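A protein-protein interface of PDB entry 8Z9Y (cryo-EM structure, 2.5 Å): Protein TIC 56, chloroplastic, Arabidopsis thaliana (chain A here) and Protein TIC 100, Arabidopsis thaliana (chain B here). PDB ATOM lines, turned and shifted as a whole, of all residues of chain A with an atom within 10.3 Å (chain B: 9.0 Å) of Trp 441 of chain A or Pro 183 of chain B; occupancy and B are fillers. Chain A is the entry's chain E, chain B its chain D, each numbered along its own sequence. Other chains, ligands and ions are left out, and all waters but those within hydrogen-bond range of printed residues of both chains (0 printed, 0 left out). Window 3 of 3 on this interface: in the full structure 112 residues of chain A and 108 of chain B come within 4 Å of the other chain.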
ATOM      1  N   PRO A 435      23.673  17.092   8.702  1.00  0.00           N
ATOM      2  CA  PRO A 435      22.926  16.779   7.480  1.00  0.00           C
ATOM      3  C   PRO A 435      22.087  17.964   7.038  1.00  0.00           C
ATOM      4  O   PRO A 435      21.378  18.575   7.851  1.00  0.00           O
ATOM      5  CB  PRO A 435      22.043  15.594   7.898  1.00  0.00           C
ATOM      6  CG  PRO A 435      22.750  14.995   9.067  1.00  0.00           C
ATOM      7  CD  PRO A 435      23.371  16.149   9.791  1.00  0.00           C
ATOM      8  N   PRO A 436      22.153  18.328   5.753  1.00  0.00           N
ATOM      9  CA  PRO A 436      21.421  19.522   5.292  1.00  0.00           C
ATOM     10  C   PRO A 436      19.912  19.430   5.445  1.00  0.00           C
ATOM     11  O   PRO A 436      19.264  20.447   5.716  1.00  0.00           O
ATOM     12  CB  PRO A 436      21.836  19.628   3.818  1.00  0.00           C
ATOM     13  CG  PRO A 436      23.138  18.903   3.736  1.00  0.00           C
ATOM     14  CD  PRO A 436      23.021  17.771   4.704  1.00  0.00           C
ATOM     15  N   TYR A 437      19.328  18.240   5.273  1.00  0.00           N
ATOM     16  CA  TYR A 437      17.873  18.128   5.278  1.00  0.00           C
ATOM     17  C   TYR A 437      17.283  18.405   6.655  1.00  0.00           C
ATOM     18  O   TYR A 437      16.124  18.829   6.761  1.00  0.00           O
ATOM     19  CB  TYR A 437      17.454  16.741   4.787  1.00  0.00           C
ATOM     20  CG  TYR A 437      17.498  15.665   5.849  1.00  0.00           C
ATOM     21  CD1 TYR A 437      18.687  15.022   6.162  1.00  0.00           C
ATOM     22  CD2 TYR A 437      16.349  15.285   6.527  1.00  0.00           C
ATOM     23  CE1 TYR A 437      18.731  14.038   7.129  1.00  0.00           C
ATOM     24  CE2 TYR A 437      16.383  14.303   7.495  1.00  0.00           C
ATOM     25  CZ  TYR A 437      17.577  13.683   7.791  1.00  0.00           C
ATOM     26  OH  TYR A 437      17.615  12.703   8.755  1.00  0.00           O
ATOM     27  N   ILE A 438      18.058  18.173   7.715  1.00  0.00           N
ATOM     28  CA  ILE A 438      17.546  18.374   9.064  1.00  0.00           C
ATOM     29  C   ILE A 438      17.245  19.846   9.316  1.00  0.00           C
ATOM     30  O   ILE A 438      16.285  20.175  10.021  1.00  0.00           O
ATOM     31  CB  ILE A 438      18.539  17.795  10.090  1.00  0.00           C
ATOM     32  CG1 ILE A 438      18.257  16.307  10.303  1.00  0.00           C
ATOM     33  CG2 ILE A 438      18.467  18.540  11.415  1.00  0.00           C
ATOM     34  CD1 ILE A 438      19.472  15.504  10.689  1.00  0.00           C
ATOM     35  N   ARG A 439      18.033  20.753   8.736  1.00  0.00           N
ATOM     36  CA  ARG A 439      17.796  22.180   8.943  1.00  0.00           C
ATOM     37  C   ARG A 439      16.457  22.615   8.352  1.00  0.00           C
ATOM     38  O   ARG A 439      15.677  23.321   9.003  1.00  0.00           O
ATOM     39  CB  ARG A 439      18.945  22.986   8.340  1.00  0.00           C
ATOM     40  CG  ARG A 439      20.259  22.226   8.287  1.00  0.00           C
ATOM     41  CD  ARG A 439      21.446  23.167   8.196  1.00  0.00           C
ATOM     42  NE  ARG A 439      21.549  24.030   9.366  1.00  0.00           N
ATOM     43  CZ  ARG A 439      21.488  25.353   9.330  1.00  0.00           C
ATOM     44  NH1 ARG A 439      21.326  26.006   8.191  1.00  0.00           N
ATOM     45  NH2 ARG A 439      21.595  26.039  10.464  1.00  0.00           N
ATOM     46  N   GLU A 440      16.166  22.198   7.117  1.00  0.00           N
ATOM     47  CA  GLU A 440      14.886  22.565   6.521  1.00  0.00           C
ATOM     48  C   GLU A 440      13.728  21.838   7.194  1.00  0.00           C
ATOM     49  O   GLU A 440      12.625  22.392   7.293  1.00  0.00           O
ATOM     50  CB  GLU A 440      14.898  22.296   5.014  1.00  0.00           C
ATOM     51  CG  GLU A 440      15.325  20.900   4.612  1.00  0.00           C
ATOM     52  CD  GLU A 440      15.194  20.662   3.120  1.00  0.00           C
ATOM     53  OE1 GLU A 440      14.116  20.958   2.562  1.00  0.00           O
ATOM     54  OE2 GLU A 440      16.167  20.179   2.505  1.00  0.00           O
ATOM     55  N   TRP A 441      13.954  20.612   7.677  1.00  0.00           N
ATOM     56  CA  TRP A 441      12.928  19.947   8.471  1.00  0.00           C
ATOM     57  C   TRP A 441      12.624  20.737   9.739  1.00  0.00           C
ATOM     58  O   TRP A 441      11.458  20.898  10.119  1.00  0.00           O
ATOM     59  CB  TRP A 441      13.370  18.524   8.810  1.00  0.00           C
ATOM     60  CG  TRP A 441      12.515  17.840   9.832  1.00  0.00           C
ATOM     61  CD1 TRP A 441      12.926  17.313  11.019  1.00  0.00           C
ATOM     62  CD2 TRP A 441      11.104  17.598   9.755  1.00  0.00           C
ATOM     63  NE1 TRP A 441      11.862  16.763  11.688  1.00  0.00           N
ATOM     64  CE2 TRP A 441      10.731  16.925  10.932  1.00  0.00           C
ATOM     65  CE3 TRP A 441      10.120  17.889   8.805  1.00  0.00           C
ATOM     66  CZ2 TRP A 441       9.419  16.536  11.187  1.00  0.00           C
ATOM     67  CZ3 TRP A 441       8.818  17.502   9.060  1.00  0.00           C
ATOM     68  CH2 TRP A 441       8.480  16.834  10.241  1.00  0.00           C
ATOM     69  N   ASN A 442      13.666  21.251  10.396  1.00  0.00           N
ATOM     70  CA  ASN A 442      13.474  22.089  11.574  1.00  0.00           C
ATOM     71  C   ASN A 442      12.709  23.356  11.227  1.00  0.00           C
ATOM     72  O   ASN A 442      11.852  23.803  11.996  1.00  0.00           O
ATOM     73  CB  ASN A 442      14.825  22.442  12.194  1.00  0.00           C
ATOM     74  CG  ASN A 442      15.475  21.265  12.887  1.00  0.00           C
ATOM     75  OD1 ASN A 442      14.841  20.237  13.117  1.00  0.00           O
ATOM     76  ND2 ASN A 442      16.751  21.411  13.223  1.00  0.00           N
ATOM     77  N   ARG A 443      13.025  23.966  10.081  1.00  0.00           N
ATOM     78  CA  ARG A 443      12.313  25.172   9.668  1.00  0.00           C
ATOM     79  C   ARG A 443      10.831  24.891   9.453  1.00  0.00           C
ATOM     80  O   ARG A 443       9.971  25.668   9.893  1.00  0.00           O
ATOM     81  CB  ARG A 443      12.942  25.748   8.400  1.00  0.00           C
ATOM     82  CG  ARG A 443      14.139  26.646   8.661  1.00  0.00           C
ATOM     83  CD  ARG A 443      14.424  27.550   7.473  1.00  0.00           C
ATOM     84  NE  ARG A 443      15.386  26.960   6.550  1.00  0.00           N
ATOM     85  CZ  ARG A 443      16.697  26.943   6.744  1.00  0.00           C
ATOM     86  NH1 ARG A 443      17.244  27.484   7.820  1.00  0.00           N
ATOM     87  NH2 ARG A 443      17.481  26.372   5.835  1.00  0.00           N
ATOM     88  N   SER A 444      10.513  23.779   8.789  1.00  0.00           N
ATOM     89  CA  SER A 444       9.113  23.401   8.611  1.00  0.00           C
ATOM     90  C   SER A 444       8.436  23.160   9.954  1.00  0.00           C
ATOM     91  O   SER A 444       7.285  23.570  10.164  1.00  0.00           O
ATOM     92  CB  SER A 444       9.013  22.156   7.730  1.00  0.00           C
ATOM     93  OG  SER A 444       9.879  22.249   6.613  1.00  0.00           O
ATOM     94  N   VAL A 445       9.137  22.496  10.876  1.00  0.00           N
ATOM     95  CA  VAL A 445       8.564  22.214  12.189  1.00  0.00           C
ATOM     96  C   VAL A 445       8.270  23.507  12.937  1.00  0.00           C
ATOM     97  O   VAL A 445       7.206  23.656  13.550  1.00  0.00           O
ATOM     98  CB  VAL A 445       9.500  21.292  12.991  1.00  0.00           C
ATOM     99  CG1 VAL A 445       9.155  21.334  14.471  1.00  0.00           C
ATOM    100  CG2 VAL A 445       9.418  19.872  12.465  1.00  0.00           C
ATOM    101  N   MET A 446       9.203  24.464  12.903  1.00  0.00           N
ATOM    102  CA  MET A 446       8.974  25.723  13.606  1.00  0.00           C
ATOM    103  C   MET A 446       7.851  26.525  12.962  1.00  0.00           C
ATOM    104  O   MET A 446       7.076  27.185  13.665  1.00  0.00           O
ATOM    105  CB  MET A 446      10.254  26.561  13.679  1.00  0.00           C
ATOM    106  CG  MET A 446      11.168  26.193  14.841  1.00  0.00           C
ATOM    107  SD  MET A 446      12.893  26.697  14.659  1.00  0.00           S
ATOM    108  CE  MET A 446      13.171  26.472  12.909  1.00  0.00           C
ATOM    109  N   ARG A 447       7.740  26.489  11.631  1.00  0.00           N
ATOM    110  CA  ARG A 447       6.625  27.172  10.981  1.00  0.00           C
ATOM    111  C   ARG A 447       5.291  26.567  11.401  1.00  0.00           C
ATOM    112  O   ARG A 447       4.338  27.295  11.716  1.00  0.00           O
ATOM    113  CB  ARG A 447       6.783  27.120   9.461  1.00  0.00           C
ATOM    114  CG  ARG A 447       7.713  28.181   8.898  1.00  0.00           C
ATOM    115  CD  ARG A 447       7.556  28.320   7.392  1.00  0.00           C
ATOM    116  NE  ARG A 447       8.283  27.291   6.660  1.00  0.00           N
ATOM    117  CZ  ARG A 447       7.725  26.204   6.143  1.00  0.00           C
ATOM    118  NH1 ARG A 447       6.428  25.973   6.255  1.00  0.00           N
ATOM    119  NH2 ARG A 447       8.488  25.329   5.494  1.00  0.00           N
ATOM    120  N   LEU A 448       5.207  25.235  11.427  1.00  0.00           N
ATOM    121  CA  LEU A 448       3.974  24.581  11.856  1.00  0.00           C
ATOM    122  C   LEU A 448       3.669  24.904  13.316  1.00  0.00           C
ATOM    123  O   LEU A 448       2.508  25.125  13.684  1.00  0.00           O
ATOM    124  CB  LEU A 448       4.090  23.070  11.630  1.00  0.00           C
ATOM    125  CG  LEU A 448       2.880  22.132  11.500  1.00  0.00           C
ATOM    126  CD1 LEU A 448       3.363  20.690  11.432  1.00  0.00           C
ATOM    127  CD2 LEU A 448       1.846  22.279  12.609  1.00  0.00           C
ATOM    128  N   PHE A 449       4.702  24.942  14.162  1.00  0.00           N
ATOM    129  CA  PHE A 449       4.500  25.279  15.567  1.00  0.00           C
ATOM    130  C   PHE A 449       3.986  26.703  15.725  1.00  0.00           C
ATOM    131  O   PHE A 449       3.114  26.965  16.561  1.00  0.00           O
ATOM    132  CB  PHE A 449       5.801  25.093  16.348  1.00  0.00           C
ATOM    133  CG  PHE A 449       5.823  25.812  17.670  1.00  0.00           C
ATOM    134  CD1 PHE A 449       5.224  25.251  18.786  1.00  0.00           C
ATOM    135  CD2 PHE A 449       6.443  27.044  17.798  1.00  0.00           C
ATOM    136  CE1 PHE A 449       5.240  25.906  20.003  1.00  0.00           C
ATOM    137  CE2 PHE A 449       6.459  27.706  19.012  1.00  0.00           C
ATOM    138  CZ  PHE A 449       5.859  27.135  20.116  1.00  0.00           C
ATOM    139  N   ARG A 450       4.532  27.644  14.950  1.00  0.00           N
ATOM    140  CA  ARG A 450       4.045  29.019  15.007  1.00  0.00           C
ATOM    141  C   ARG A 450       2.600  29.108  14.539  1.00  0.00           C
ATOM    142  O   ARG A 450       1.808  29.879  15.091  1.00  0.00           O
ATOM    143  CB  ARG A 450       4.938  29.937  14.174  1.00  0.00           C
ATOM    144  CG  ARG A 450       6.258  30.290  14.833  1.00  0.00           C
ATOM    145  CD  ARG A 450       6.975  31.384  14.062  1.00  0.00           C
ATOM    146  NE  ARG A 450       8.352  31.556  14.508  1.00  0.00           N
ATOM    147  CZ  ARG A 450       9.411  31.062  13.881  1.00  0.00           C
ATOM    148  NH1 ARG A 450       9.287  30.355  12.770  1.00  0.00           N
ATOM    149  NH2 ARG A 450      10.623  31.283  14.381  1.00  0.00           N
ATOM    150  N   TYR B 109      10.372   4.824  19.299  1.00  0.00           N
ATOM    151  CA  TYR B 109      11.119   5.413  18.194  1.00  0.00           C
ATOM    152  C   TYR B 109      12.418   4.662  17.935  1.00  0.00           C
ATOM    153  O   TYR B 109      12.909   4.644  16.800  1.00  0.00           O
ATOM    154  CB  TYR B 109      11.403   6.888  18.481  1.00  0.00           C
ATOM    155  CG  TYR B 109      11.931   7.659  17.294  1.00  0.00           C
ATOM    156  CD1 TYR B 109      11.066   8.194  16.350  1.00  0.00           C
ATOM    157  CD2 TYR B 109      13.294   7.858  17.119  1.00  0.00           C
ATOM    158  CE1 TYR B 109      11.541   8.902  15.265  1.00  0.00           C
ATOM    159  CE2 TYR B 109      13.778   8.564  16.036  1.00  0.00           C
ATOM    160  CZ  TYR B 109      12.898   9.084  15.113  1.00  0.00           C
ATOM    161  OH  TYR B 109      13.377   9.788  14.033  1.00  0.00           O
ATOM    162  N   PHE B 113      14.815   1.616  14.219  1.00  0.00           N
ATOM    163  CA  PHE B 113      16.179   1.755  13.723  1.00  0.00           C
ATOM    164  C   PHE B 113      17.060   0.547  14.013  1.00  0.00           C
ATOM    165  O   PHE B 113      18.284   0.644  13.868  1.00  0.00           O
ATOM    166  CB  PHE B 113      16.821   3.014  14.308  1.00  0.00           C
ATOM    167  CG  PHE B 113      16.551   4.254  13.512  1.00  0.00           C
ATOM    168  CD1 PHE B 113      17.048   4.388  12.227  1.00  0.00           C
ATOM    169  CD2 PHE B 113      15.797   5.283  14.044  1.00  0.00           C
ATOM    170  CE1 PHE B 113      16.799   5.527  11.491  1.00  0.00           C
ATOM    171  CE2 PHE B 113      15.545   6.424  13.313  1.00  0.00           C
ATOM    172  CZ  PHE B 113      16.047   6.545  12.035  1.00  0.00           C
ATOM    173  N   PRO B 180      18.502   9.847  14.141  1.00  0.00           N
ATOM    174  CA  PRO B 180      18.137  10.815  13.100  1.00  0.00           C
ATOM    175  C   PRO B 180      16.628  10.958  12.977  1.00  0.00           C
ATOM    176  O   PRO B 180      15.869  10.011  13.194  1.00  0.00           O
ATOM    177  CB  PRO B 180      18.748  10.219  11.825  1.00  0.00           C
ATOM    178  CG  PRO B 180      19.714   9.183  12.293  1.00  0.00           C
ATOM    179  CD  PRO B 180      19.179   8.668  13.583  1.00  0.00           C
ATOM    180  N   ALA B 181      16.197  12.164  12.622  1.00  0.00           N
ATOM    181  CA  ALA B 181      14.780  12.448  12.470  1.00  0.00           C
ATOM    182  C   ALA B 181      14.290  12.023  11.092  1.00  0.00           C
ATOM    183  O   ALA B 181      15.021  12.085  10.101  1.00  0.00           O
ATOM    184  CB  ALA B 181      14.503  13.936  12.686  1.00  0.00           C
ATOM    185  N   ILE B 182      13.036  11.587  11.039  1.00  0.00           N
ATOM    186  CA  ILE B 182      12.394  11.166   9.801  1.00  0.00           C
ATOM    187  C   ILE B 182      11.383  12.242   9.413  1.00  0.00           C
ATOM    188  O   ILE B 182      10.322  12.351  10.045  1.00  0.00           O
ATOM    189  CB  ILE B 182      11.718   9.796   9.947  1.00  0.00           C
ATOM    190  CG1 ILE B 182      12.732   8.748  10.407  1.00  0.00           C
ATOM    191  CG2 ILE B 182      11.081   9.375   8.635  1.00  0.00           C
ATOM    192  CD1 ILE B 182      12.100   7.497  10.968  1.00  0.00           C
ATOM    193  N   PRO B 183      11.660  13.056   8.392  1.00  0.00           N
ATOM    194  CA  PRO B 183      10.720  14.114   7.996  1.00  0.00           C
ATOM    195  C   PRO B 183       9.634  13.556   7.089  1.00  0.00           C
ATOM    196  O   PRO B 183       9.925  12.947   6.057  1.00  0.00           O
ATOM    197  CB  PRO B 183      11.613  15.118   7.257  1.00  0.00           C
ATOM    198  CG  PRO B 183      12.724  14.286   6.699  1.00  0.00           C
ATOM    199  CD  PRO B 183      12.889  13.068   7.578  1.00  0.00           C
ATOM    200  N   ASP B 184       8.378  13.756   7.477  1.00  0.00           N
ATOM    201  CA  ASP B 184       7.254  13.264   6.682  1.00  0.00           C
ATOM    202  C   ASP B 184       6.750  14.321   5.701  1.00  0.00           C
ATOM    203  O   ASP B 184       5.552  14.575   5.591  1.00  0.00           O
ATOM    204  CB  ASP B 184       6.134  12.802   7.606  1.00  0.00           C
ATOM    205  CG  ASP B 184       6.649  12.030   8.802  1.00  0.00           C
ATOM    206  OD1 ASP B 184       7.750  11.449   8.705  1.00  0.00           O
ATOM    207  OD2 ASP B 184       5.952  12.000   9.838  1.00  0.00           O
ATOM    208  N   ASN B 185       7.677  14.947   4.977  1.00  0.00           N
ATOM    209  CA  ASN B 185       7.318  15.854   3.893  1.00  0.00           C
ATOM    210  C   ASN B 185       8.208  15.734   2.666  1.00  0.00           C
ATOM    211  O   ASN B 185       7.836  16.259   1.612  1.00  0.00           O
ATOM    212  CB  ASN B 185       7.338  17.311   4.381  1.00  0.00           C
ATOM    213  CG  ASN B 185       8.734  17.793   4.730  1.00  0.00           C
ATOM    214  OD1 ASN B 185       9.645  16.996   4.952  1.00  0.00           O
ATOM    215  ND2 ASN B 185       8.907  19.109   4.779  1.00  0.00           N
ATOM    216  N   HIS B 186       9.361  15.069   2.758  1.00  0.00           N
ATOM    217  CA  HIS B 186      10.354  15.125   1.693  1.00  0.00           C
ATOM    218  C   HIS B 186       9.988  14.252   0.500  1.00  0.00           C
ATOM    219  O   HIS B 186      10.440  14.530  -0.617  1.00  0.00           O
ATOM    220  CB  HIS B 186      11.723  14.714   2.238  1.00  0.00           C
ATOM    221  CG  HIS B 186      12.875  15.256   1.450  1.00  0.00           C
ATOM    222  ND1 HIS B 186      13.009  15.056   0.093  1.00  0.00           N
ATOM    223  CD2 HIS B 186      13.947  15.989   1.831  1.00  0.00           C
ATOM    224  CE1 HIS B 186      14.114  15.643  -0.328  1.00  0.00           C
ATOM    225  NE2 HIS B 186      14.702  16.217   0.706  1.00  0.00           N
ATOM    226  N   TYR B 187       9.216  13.183   0.721  1.00  0.00           N
ATOM    227  CA  TYR B 187       8.837  12.215  -0.308  1.00  0.00           C
ATOM    228  C   TYR B 187      10.044  11.404  -0.772  1.00  0.00           C
ATOM    229  O   TYR B 187       9.904  10.459  -1.556  1.00  0.00           O
ATOM    230  CB  TYR B 187       8.158  12.915  -1.495  1.00  0.00           C
ATOM    231  CG  TYR B 187       7.685  11.984  -2.590  1.00  0.00           C
ATOM    232  CD1 TYR B 187       6.551  11.201  -2.424  1.00  0.00           C
ATOM    233  CD2 TYR B 187       8.373  11.892  -3.794  1.00  0.00           C
ATOM    234  CE1 TYR B 187       6.118  10.349  -3.425  1.00  0.00           C
ATOM    235  CE2 TYR B 187       7.949  11.045  -4.798  1.00  0.00           C
ATOM    236  CZ  TYR B 187       6.821  10.277  -4.609  1.00  0.00           C
ATOM    237  OH  TYR B 187       6.395   9.432  -5.608  1.00  0.00           O
ATOM    238  N   ASP B 188      11.229  11.740  -0.270  1.00  0.00           N
ATOM    239  CA  ASP B 188      12.449  11.020  -0.599  1.00  0.00           C
ATOM    240  C   ASP B 188      12.944  10.143   0.539  1.00  0.00           C
ATOM    241  O   ASP B 188      13.919   9.408   0.355  1.00  0.00           O
ATOM    242  CB  ASP B 188      13.552  12.002  -1.004  1.00  0.00           C
ATOM    243  CG  ASP B 188      13.668  12.162  -2.505  1.00  0.00           C
ATOM    244  OD1 ASP B 188      13.325  11.208  -3.234  1.00  0.00           O
ATOM    245  OD2 ASP B 188      14.103  13.242  -2.957  1.00  0.00           O
ATOM    246  N   ILE B 189      12.307  10.198   1.709  1.00  0.00           N
ATOM    247  CA  ILE B 189      12.774   9.413   2.844  1.00  0.00           C
ATOM    248  C   ILE B 189      11.736   8.366   3.222  1.00  0.00           C
ATOM    249  O   ILE B 189      11.971   7.162   3.071  1.00  0.00           O
ATOM    250  CB  ILE B 189      13.082  10.326   4.045  1.00  0.00           C
ATOM    251  CG1 ILE B 189      13.837  11.579   3.594  1.00  0.00           C
ATOM    252  CG2 ILE B 189      13.862   9.571   5.094  1.00  0.00           C
ATOM    253  CD1 ILE B 189      15.184  11.295   2.980  1.00  0.00           C
ATOM    254  N   GLU B 190      10.589   8.821   3.735  1.00  0.00           N
ATOM    255  CA  GLU B 190       9.397   8.006   3.957  1.00  0.00           C
ATOM    256  C   GLU B 190       9.636   6.804   4.871  1.00  0.00           C
ATOM    257  O   GLU B 190       8.705   6.039   5.147  1.00  0.00           O
ATOM    258  CB  GLU B 190       8.815   7.555   2.608  1.00  0.00           C
ATOM    259  CG  GLU B 190       9.217   6.163   2.140  1.00  0.00           C
ATOM    260  CD  GLU B 190       8.888   5.926   0.680  1.00  0.00           C
ATOM    261  OE1 GLU B 190       8.393   6.865   0.022  1.00  0.00           O
ATOM    262  OE2 GLU B 190       9.127   4.804   0.190  1.00  0.00           O
ATOM    263  N   ASN B 191      10.854   6.646   5.383  1.00  0.00           N
ATOM    264  CA  ASN B 191      11.236   5.430   6.087  1.00  0.00           C
ATOM    265  C   ASN B 191      12.513   5.698   6.874  1.00  0.00           C
ATOM    266  O   ASN B 191      13.048   6.809   6.869  1.00  0.00           O
ATOM    267  CB  ASN B 191      11.427   4.270   5.105  1.00  0.00           C
ATOM    268  CG  ASN B 191      10.597   3.057   5.464  1.00  0.00           C
ATOM    269  OD1 ASN B 191       9.541   3.174   6.084  1.00  0.00           O
ATOM    270  ND2 ASN B 191      11.071   1.880   5.071  1.00  0.00           N
ATOM    271  N   ALA B 192      12.997   4.661   7.558  1.00  0.00           N
ATOM    272  CA  ALA B 192      14.287   4.714   8.235  1.00  0.00           C
ATOM    273  C   ALA B 192      15.431   4.341   7.301  1.00  0.00           C
ATOM    274  O   ALA B 192      16.495   4.971   7.336  1.00  0.00           O
ATOM    275  CB  ALA B 192      14.282   3.790   9.454  1.00  0.00           C
ATOM    276  N   GLY B 194      15.226   5.008   4.304  1.00  0.00           N
ATOM    277  CA  GLY B 194      15.324   6.261   3.576  1.00  0.00           C
ATOM    278  C   GLY B 194      16.296   7.229   4.223  1.00  0.00           C
ATOM    279  O   GLY B 194      17.089   7.873   3.538  1.00  0.00           O
ATOM    280  N   VAL B 195      16.253   7.334   5.554  1.00  0.00           N
ATOM    281  CA  VAL B 195      17.211   8.178   6.268  1.00  0.00           C
ATOM    282  C   VAL B 195      18.628   7.661   6.060  1.00  0.00           C
ATOM    283  O   VAL B 195      19.566   8.439   5.837  1.00  0.00           O
ATOM    284  CB  VAL B 195      16.851   8.250   7.765  1.00  0.00           C
ATOM    285  CG1 VAL B 195      18.091   8.506   8.606  1.00  0.00           C
ATOM    286  CG2 VAL B 195      15.818   9.331   8.016  1.00  0.00           C
ATOM    287  N   GLU B 198      19.737   8.517   2.643  1.00  0.00           N
ATOM    288  CA  GLU B 198      19.919   9.958   2.519  1.00  0.00           C
ATOM    289  C   GLU B 198      21.223  10.410   3.158  1.00  0.00           C
ATOM    290  O   GLU B 198      21.852  11.359   2.676  1.00  0.00           O
ATOM    291  CB  GLU B 198      18.728  10.680   3.150  1.00  0.00           C
ATOM    292  CG  GLU B 198      18.991  12.118   3.561  1.00  0.00           C
ATOM    293  CD  GLU B 198      19.030  13.063   2.379  1.00  0.00           C
ATOM    294  OE1 GLU B 198      18.012  13.164   1.664  1.00  0.00           O
ATOM    295  OE2 GLU B 198      20.078  13.708   2.165  1.00  0.00           O
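Printed residues of chain B within 4 Å of Trp 441 of chain A: Ala 181, Pro 183 and Asn 185. Of the printed residues of chain A, Pro 183 of chain B touches Tyr 437 and Trp 441. No residue of chain A comes within 4 Å of Asp 184 of chain B. Of the printed residues of chain B, Tyr 437 of chain A touches Ala 181, Pro 183, Val 195 and Glu 198. Of the printed residues of chain B, Ser 444 of chain A touches Asn 185. Of the printed residues of chain A, Ala 181 of chain B touches Tyr 437 (3.0 Å) and Trp 441 (3.995 Å). Printed residues of chain A within 4 Å of Asn 185 of chain B: Trp 441 (3.98 Å) and Ser 444 (3.8 Å). Tyr 109 of chain B touches none of the printed residues of chain A. Asn 191 of chain B touches none of the printed residues of chain A. The nearest printed residue of chain B that does not touch Trp 441 of chain A is Asp 184 of chain B (4.1 Å). The nearest residue of chain A that does not touch Pro 183 of chain B is Ile 438 of chain A (6.7 Å). The nearest printed residue of chain A that does not touch Ala 181 of chain B is Ile 438 of chain A (5.0 Å).
OG of Ser 444 of chain A lies within hydrogen-bond range of O of Glu 440 of chain A (2.8 Å).
OH of Tyr 437 of chain A sits at hydrogen-bond distance from O of Ala 181 of chain B, at 3.0 Å.
Of the 18 printed residues of chain B, 5 touch a printed residue of chain A. Hydrophobic or aromatic side chains of chain B that line the printed part of chain A: Ala 181, Pro 183 and Val 195. Hydrophobic or aromatic side chains of chain A that line the printed part of chain B: Tyr 437 and Trp 441. Among the printed residues, 8 pairs touch across the chains. Among the printed residues, no Asp or Glu carboxylate lies within 4 Å of a Lys or Arg side-chain nitrogen of the other chain.
Tyr 437 of chain A touches Pro 183 of chain B. Val 195 of chain B touches Tyr 437 of chain A. Tyr 437 of chain A touches Glu 198 of chain B (CD1 to CG, 3.9 Å). Trp 441 of chain A touches Ala 181 of chain B. Pro 183 of chain B touches Trp 441 of chain A (CB to CE3, 3.5 Å). OD1 of Asn 185 of chain B touches CE3 of Trp 441 of chain A (3.98 Å). Ser 444 of chain A touches Asn 185 of chain B.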
